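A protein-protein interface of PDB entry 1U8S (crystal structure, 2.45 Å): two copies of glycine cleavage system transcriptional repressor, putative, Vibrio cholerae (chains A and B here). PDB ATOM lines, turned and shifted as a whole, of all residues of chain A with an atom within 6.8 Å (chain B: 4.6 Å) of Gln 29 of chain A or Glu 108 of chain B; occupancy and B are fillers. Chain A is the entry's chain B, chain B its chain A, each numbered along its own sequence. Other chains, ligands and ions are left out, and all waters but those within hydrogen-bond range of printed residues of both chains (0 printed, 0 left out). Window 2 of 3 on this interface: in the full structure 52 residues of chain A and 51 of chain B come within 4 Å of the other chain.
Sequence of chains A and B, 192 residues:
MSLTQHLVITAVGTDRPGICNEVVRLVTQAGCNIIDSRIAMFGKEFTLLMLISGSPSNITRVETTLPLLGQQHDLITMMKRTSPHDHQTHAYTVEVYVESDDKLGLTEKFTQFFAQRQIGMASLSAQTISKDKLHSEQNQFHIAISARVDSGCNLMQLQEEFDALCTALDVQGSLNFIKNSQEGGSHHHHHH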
ATOM      1  N   ASN A  21      22.064  15.149   3.089  1.00  0.00           N
ATOM      2  CA  ASN A  21      21.616  13.987   3.850  1.00  0.00           C
ATOM      3  C   ASN A  21      22.403  12.768   3.400  1.00  0.00           C
ATOM      4  O   ASN A  21      23.058  12.103   4.196  1.00  0.00           O
ATOM      5  CB  ASN A  21      20.127  13.718   3.614  1.00  0.00           C
ATOM      6  CG  ASN A  21      19.237  14.418   4.621  1.00  0.00           C
ATOM      7  OD1 ASN A  21      18.125  14.841   4.293  1.00  0.00           O
ATOM      8  ND2 ASN A  21      19.709  14.527   5.859  1.00  0.00           N
ATOM      9  N   GLU A  22      22.334  12.492   2.105  1.00  0.00           N
ATOM     10  CA  GLU A  22      23.011  11.345   1.518  1.00  0.00           C
ATOM     11  C   GLU A  22      24.501  11.342   1.809  1.00  0.00           C
ATOM     12  O   GLU A  22      25.089  10.286   2.047  1.00  0.00           O
ATOM     13  CB  GLU A  22      22.769  11.335   0.010  1.00  0.00           C
ATOM     14  CG  GLU A  22      21.293  11.393  -0.352  1.00  0.00           C
ATOM     15  CD  GLU A  22      21.053  11.869  -1.772  1.00  0.00           C
ATOM     16  OE1 GLU A  22      19.884  12.155  -2.112  1.00  0.00           O
ATOM     17  OE2 GLU A  22      22.031  11.955  -2.547  1.00  0.00           O
ATOM     18  N   VAL A  23      25.114  12.519   1.799  1.00  0.00           N
ATOM     19  CA  VAL A  23      26.542  12.607   2.062  1.00  0.00           C
ATOM     20  C   VAL A  23      26.895  12.110   3.452  1.00  0.00           C
ATOM     21  O   VAL A  23      27.722  11.210   3.599  1.00  0.00           O
ATOM     22  CB  VAL A  23      27.054  14.037   1.900  1.00  0.00           C
ATOM     23  CG1 VAL A  23      28.542  14.084   2.196  1.00  0.00           C
ATOM     24  CG2 VAL A  23      26.789  14.517   0.484  1.00  0.00           C
ATOM     25  N   VAL A  24      26.278  12.680   4.478  1.00  0.00           N
ATOM     26  CA  VAL A  24      26.577  12.242   5.839  1.00  0.00           C
ATOM     27  C   VAL A  24      26.011  10.847   6.049  1.00  0.00           C
ATOM     28  O   VAL A  24      26.470  10.092   6.907  1.00  0.00           O
ATOM     29  CB  VAL A  24      25.966  13.189   6.910  1.00  0.00           C
ATOM     30  CG1 VAL A  24      26.384  14.619   6.637  1.00  0.00           C
ATOM     31  CG2 VAL A  24      24.456  13.056   6.933  1.00  0.00           C
ATOM     32  N   ARG A  25      25.003  10.521   5.249  1.00  0.00           N
ATOM     33  CA  ARG A  25      24.335   9.229   5.318  1.00  0.00           C
ATOM     34  C   ARG A  25      25.305   8.152   4.862  1.00  0.00           C
ATOM     35  O   ARG A  25      25.522   7.153   5.546  1.00  0.00           O
ATOM     36  CB  ARG A  25      23.094   9.255   4.418  1.00  0.00           C
ATOM     37  CG  ARG A  25      22.288   7.973   4.375  1.00  0.00           C
ATOM     38  CD  ARG A  25      21.036   8.149   3.518  1.00  0.00           C
ATOM     39  NE  ARG A  25      20.435   6.862   3.190  1.00  0.00           N
ATOM     40  CZ  ARG A  25      21.050   5.914   2.491  1.00  0.00           C
ATOM     41  NH1 ARG A  25      22.286   6.111   2.042  1.00  0.00           N
ATOM     42  NH2 ARG A  25      20.438   4.763   2.242  1.00  0.00           N
ATOM     43  N   LEU A  26      25.893   8.384   3.698  1.00  0.00           N
ATOM     44  CA  LEU A  26      26.844   7.461   3.106  1.00  0.00           C
ATOM     45  C   LEU A  26      28.071   7.320   4.003  1.00  0.00           C
ATOM     46  O   LEU A  26      28.580   6.217   4.209  1.00  0.00           O
ATOM     47  CB  LEU A  26      27.242   7.974   1.717  1.00  0.00           C
ATOM     48  CG  LEU A  26      28.054   7.073   0.789  1.00  0.00           C
ATOM     49  CD1 LEU A  26      27.847   7.526  -0.650  1.00  0.00           C
ATOM     50  CD2 LEU A  26      29.525   7.114   1.172  1.00  0.00           C
ATOM     51  N   VAL A  27      28.529   8.443   4.546  1.00  0.00           N
ATOM     52  CA  VAL A  27      29.701   8.458   5.418  1.00  0.00           C
ATOM     53  C   VAL A  27      29.488   7.759   6.760  1.00  0.00           C
ATOM     54  O   VAL A  27      30.284   6.896   7.151  1.00  0.00           O
ATOM     55  CB  VAL A  27      30.172   9.908   5.677  1.00  0.00           C
ATOM     56  CG1 VAL A  27      31.260   9.931   6.728  1.00  0.00           C
ATOM     57  CG2 VAL A  27      30.693  10.506   4.390  1.00  0.00           C
ATOM     58  N   THR A  28      28.428   8.133   7.471  1.00  0.00           N
ATOM     59  CA  THR A  28      28.150   7.528   8.769  1.00  0.00           C
ATOM     60  C   THR A  28      27.754   6.068   8.609  1.00  0.00           C
ATOM     61  O   THR A  28      28.164   5.224   9.408  1.00  0.00           O
ATOM     62  CB  THR A  28      27.023   8.272   9.512  1.00  0.00           C
ATOM     63  OG1 THR A  28      25.834   8.252   8.716  1.00  0.00           O
ATOM     64  CG2 THR A  28      27.430   9.707   9.785  1.00  0.00           C
ATOM     65  N   GLN A  29      26.965   5.778   7.572  1.00  0.00           N
ATOM     66  CA  GLN A  29      26.521   4.410   7.293  1.00  0.00           C
ATOM     67  C   GLN A  29      27.662   3.539   6.747  1.00  0.00           C
ATOM     68  O   GLN A  29      27.463   2.364   6.434  1.00  0.00           O
ATOM     69  CB  GLN A  29      25.342   4.416   6.303  1.00  0.00           C
ATOM     70  CG  GLN A  29      23.985   4.750   6.941  1.00  0.00           C
ATOM     71  CD  GLN A  29      22.801   4.469   6.017  1.00  0.00           C
ATOM     72  OE1 GLN A  29      22.791   3.473   5.290  1.00  0.00           O
ATOM     73  NE2 GLN A  29      21.793   5.336   6.056  1.00  0.00           N
ATOM     74  N   ALA A  30      28.853   4.123   6.634  1.00  0.00           N
ATOM     75  CA  ALA A  30      30.027   3.403   6.149  1.00  0.00           C
ATOM     76  C   ALA A  30      30.898   2.990   7.333  1.00  0.00           C
ATOM     77  O   ALA A  30      31.872   2.252   7.175  1.00  0.00           O
ATOM     78  CB  ALA A  30      30.827   4.277   5.194  1.00  0.00           C
ATOM     79  N   GLY A  31      30.542   3.479   8.518  1.00  0.00           N
ATOM     80  CA  GLY A  31      31.285   3.154   9.722  1.00  0.00           C
ATOM     81  C   GLY A  31      32.247   4.242  10.158  1.00  0.00           C
ATOM     82  O   GLY A  31      32.882   4.139  11.208  1.00  0.00           O
ATOM     83  N   CYS A  32      32.353   5.297   9.359  1.00  0.00           N
ATOM     84  CA  CYS A  32      33.261   6.381   9.679  1.00  0.00           C
ATOM     85  C   CYS A  32      32.665   7.438  10.597  1.00  0.00           C
ATOM     86  O   CYS A  32      31.451   7.538  10.762  1.00  0.00           O
ATOM     87  CB  CYS A  32      33.743   7.041   8.394  1.00  0.00           C
ATOM     88  SG  CYS A  32      34.507   5.891   7.250  1.00  0.00           S
ATOM     89  N   ARG A  61      35.577   1.873   1.843  1.00  0.00           N
ATOM     90  CA  ARG A  61      34.151   1.788   1.548  1.00  0.00           C
ATOM     91  C   ARG A  61      33.636   3.159   1.156  1.00  0.00           C
ATOM     92  O   ARG A  61      32.802   3.280   0.264  1.00  0.00           O
ATOM     93  CB  ARG A  61      33.370   1.298   2.762  1.00  0.00           C
ATOM     94  CG  ARG A  61      31.858   1.390   2.588  1.00  0.00           C
ATOM     95  CD  ARG A  61      31.328   0.348   1.611  1.00  0.00           C
ATOM     96  NE  ARG A  61      29.899   0.524   1.338  1.00  0.00           N
ATOM     97  CZ  ARG A  61      29.114  -0.422   0.825  1.00  0.00           C
ATOM     98  NH1 ARG A  61      29.622  -1.614   0.534  1.00  0.00           N
ATOM     99  NH2 ARG A  61      27.824  -0.180   0.602  1.00  0.00           N
ATOM    100  N   GLY B 105      22.209   5.287  12.250  1.00  0.00           N
ATOM    101  CA  GLY B 105      21.364   6.267  11.576  1.00  0.00           C
ATOM    102  C   GLY B 105      20.861   7.466  12.358  1.00  0.00           C
ATOM    103  O   GLY B 105      19.782   7.989  12.086  1.00  0.00           O
ATOM    104  N   LEU B 106      21.649   7.921  13.319  1.00  0.00           N
ATOM    105  CA  LEU B 106      21.263   9.048  14.140  1.00  0.00           C
ATOM    106  C   LEU B 106      21.552  10.358  13.415  1.00  0.00           C
ATOM    107  O   LEU B 106      20.731  11.281  13.427  1.00  0.00           O
ATOM    108  CB  LEU B 106      22.024   8.972  15.463  1.00  0.00           C
ATOM    109  CG  LEU B 106      21.593   9.878  16.616  1.00  0.00           C
ATOM    110  CD1 LEU B 106      20.115   9.682  16.926  1.00  0.00           C
ATOM    111  CD2 LEU B 106      22.437   9.553  17.837  1.00  0.00           C
ATOM    112  N   THR B 107      22.708  10.434  12.765  1.00  0.00           N
ATOM    113  CA  THR B 107      23.079  11.645  12.051  1.00  0.00           C
ATOM    114  C   THR B 107      22.056  12.114  11.013  1.00  0.00           C
ATOM    115  O   THR B 107      21.592  13.248  11.088  1.00  0.00           O
ATOM    116  CB  THR B 107      24.447  11.493  11.368  1.00  0.00           C
ATOM    117  OG1 THR B 107      25.420  11.116  12.345  1.00  0.00           O
ATOM    118  CG2 THR B 107      24.876  12.815  10.737  1.00  0.00           C
ATOM    119  N   GLU B 108      21.701  11.268  10.050  1.00  0.00           N
ATOM    120  CA  GLU B 108      20.730  11.691   9.040  1.00  0.00           C
ATOM    121  C   GLU B 108      19.489  12.312   9.675  1.00  0.00           C
ATOM    122  O   GLU B 108      18.894  13.225   9.114  1.00  0.00           O
ATOM    123  CB  GLU B 108      20.269  10.520   8.160  1.00  0.00           C
ATOM    124  CG  GLU B 108      21.370   9.665   7.571  1.00  0.00           C
ATOM    125  CD  GLU B 108      21.837   8.584   8.535  1.00  0.00           C
ATOM    126  OE1 GLU B 108      22.344   8.929   9.627  1.00  0.00           O
ATOM    127  OE2 GLU B 108      21.695   7.389   8.196  1.00  0.00           O
ATOM    128  N   LYS B 109      19.092  11.815  10.839  1.00  0.00           N
ATOM    129  CA  LYS B 109      17.902  12.336  11.501  1.00  0.00           C
ATOM    130  C   LYS B 109      17.974  13.834  11.757  1.00  0.00           C
ATOM    131  O   LYS B 109      17.026  14.584  11.480  1.00  0.00           O
ATOM    132  CB  LYS B 109      17.655  11.613  12.830  1.00  0.00           C
ATOM    133  CG  LYS B 109      16.653  10.468  12.755  1.00  0.00           C
ATOM    134  CD  LYS B 109      17.136   9.336  11.864  1.00  0.00           C
ATOM    135  CE  LYS B 109      16.303   8.076  12.067  1.00  0.00           C
ATOM    136  NZ  LYS B 109      16.891   6.932  11.329  1.00  0.00           N
ATOM    137  N   PHE B 110      19.111  14.278  12.267  1.00  0.00           N
ATOM    138  CA  PHE B 110      19.262  15.679  12.575  1.00  0.00           C
ATOM    139  C   PHE B 110      19.505  16.575  11.364  1.00  0.00           C
ATOM    140  O   PHE B 110      19.054  17.718  11.335  1.00  0.00           O
ATOM    141  CB  PHE B 110      20.337  15.823  13.641  1.00  0.00           C
ATOM    142  CG  PHE B 110      19.907  15.287  14.984  1.00  0.00           C
ATOM    143  CD1 PHE B 110      19.235  16.098  15.888  1.00  0.00           C
ATOM    144  CD2 PHE B 110      20.117  13.958  15.318  1.00  0.00           C
ATOM    145  CE1 PHE B 110      18.777  15.589  17.097  1.00  0.00           C
ATOM    146  CE2 PHE B 110      19.659  13.444  16.526  1.00  0.00           C
ATOM    147  CZ  PHE B 110      18.991  14.259  17.414  1.00  0.00           C
ATOM    148  N   THR B 111      20.198  16.070  10.351  1.00  0.00           N
ATOM    149  CA  THR B 111      20.414  16.885   9.169  1.00  0.00           C
ATOM    150  C   THR B 111      19.061  17.026   8.490  1.00  0.00           C
ATOM    151  O   THR B 111      18.685  18.114   8.069  1.00  0.00           O
ATOM    152  CB  THR B 111      21.449  16.256   8.213  1.00  0.00           C
ATOM    153  OG1 THR B 111      21.190  14.860   8.059  1.00  0.00           O
ATOM    154  CG2 THR B 111      22.853  16.460   8.764  1.00  0.00           C
ATOM    155  N   GLN B 112      18.316  15.933   8.405  1.00  0.00           N
ATOM    156  CA  GLN B 112      16.990  15.994   7.806  1.00  0.00           C
ATOM    157  C   GLN B 112      16.132  17.000   8.603  1.00  0.00           C
ATOM    158  O   GLN B 112      15.458  17.855   8.028  1.00  0.00           O
ATOM    159  CB  GLN B 112      16.344  14.606   7.815  1.00  0.00           C
ATOM    160  CG  GLN B 112      14.855  14.607   7.468  1.00  0.00           C
ATOM    161  CD  GLN B 112      14.565  15.207   6.099  1.00  0.00           C
ATOM    162  OE1 GLN B 112      13.420  15.554   5.793  1.00  0.00           O
ATOM    163  NE2 GLN B 112      15.600  15.327   5.264  1.00  0.00           N
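Among the printed residues, pairs that only touch across the chains: Thr 28 of chain A with Thr 107 of chain B (3.5 Å), Asn 21 of chain A with Glu 108 of chain B (3.6 Å), Arg 25 of chain A with Glu 108 of chain B (3.6 Å), Thr 28 of chain A with Glu 108 of chain B (3.7 Å), Val 24 of chain A with Thr 107 of chain B (3.8 Å) and Val 24 of chain A with Thr 111 of chain B (3.9 Å).
O of Thr 107 of chain B lies within hydrogen-bond range of OG1 of Thr 111 of chain B (3.5 Å). The backbone carbonyl oxygen (O) of Glu 108 of chain B is in hydrogen-bond range of the side-chain hydroxyl (OG1) of Thr 111 of chain B. The side-chain hydroxyl (OG1) of Thr 28 of chain A sits at hydrogen-bond distance from the backbone carbonyl oxygen (O) of Arg 25 of chain A (3.4 Å). O of Val 24 of chain A lies within hydrogen-bond range of OG1 of Thr 28 of chain A.
Hydrophobic or aromatic side chains of chain A that line the printed part of chain B: Val 24. Among the printed residues, no Asp or Glu carboxylate lies within 4 Å of a Lys or Arg side-chain nitrogen of the other chain.
Printed residues of chain B within 4 Å of Val 24 of chain A: Thr 107 (3.8 Å) and Thr 111 (3.9 Å). Of the printed residues of chain B, Arg 25 of chain A touches Glu 108 (3.6 Å). Gln 29 of chain A touches just one residue of chain B: Glu 108 (3.0 Å). Printed residues of chain A within 4 Å of Thr 107 of chain B: Val 24 (3.8 Å) and Thr 28 (3.5 Å). Of chain A, only Asn 21 (3.6 Å), Arg 25 (3.6 Å), Thr 28 (3.7 Å) and Gln 29 (3.0 Å) come within 4 Å of Glu 108 of chain B. Of the printed residues of chain A, Thr 111 of chain B touches Asn 21 and Val 24. Printed residues of chain A within 4 Å of Gln 112 of chain B: Asn 21 (2.7 Å). The nearest printed residue of chain B that does not touch Gln 29 of chain A is Gly 105 of chain B (5.5 Å).
NE2 of Gln 112 of chain B is in hydrogen-bond range of OD1 of Asn 21 of chain A (2.7 Å). NE2 of Gln 29 of chain A lies within hydrogen-bond range of OE2 of Glu 108 of chain B (3.0 Å). The side-chain hydroxyl of Thr 111 of chain B lies within hydrogen-bond range of the side-chain amide nitrogen of Asn 21 of chain A, at 2.7 Å.
No position is printed for both chains. Of the 9 pairs that touch across the chains among the printed residues, none has its exchanged pair printed and touching as well.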
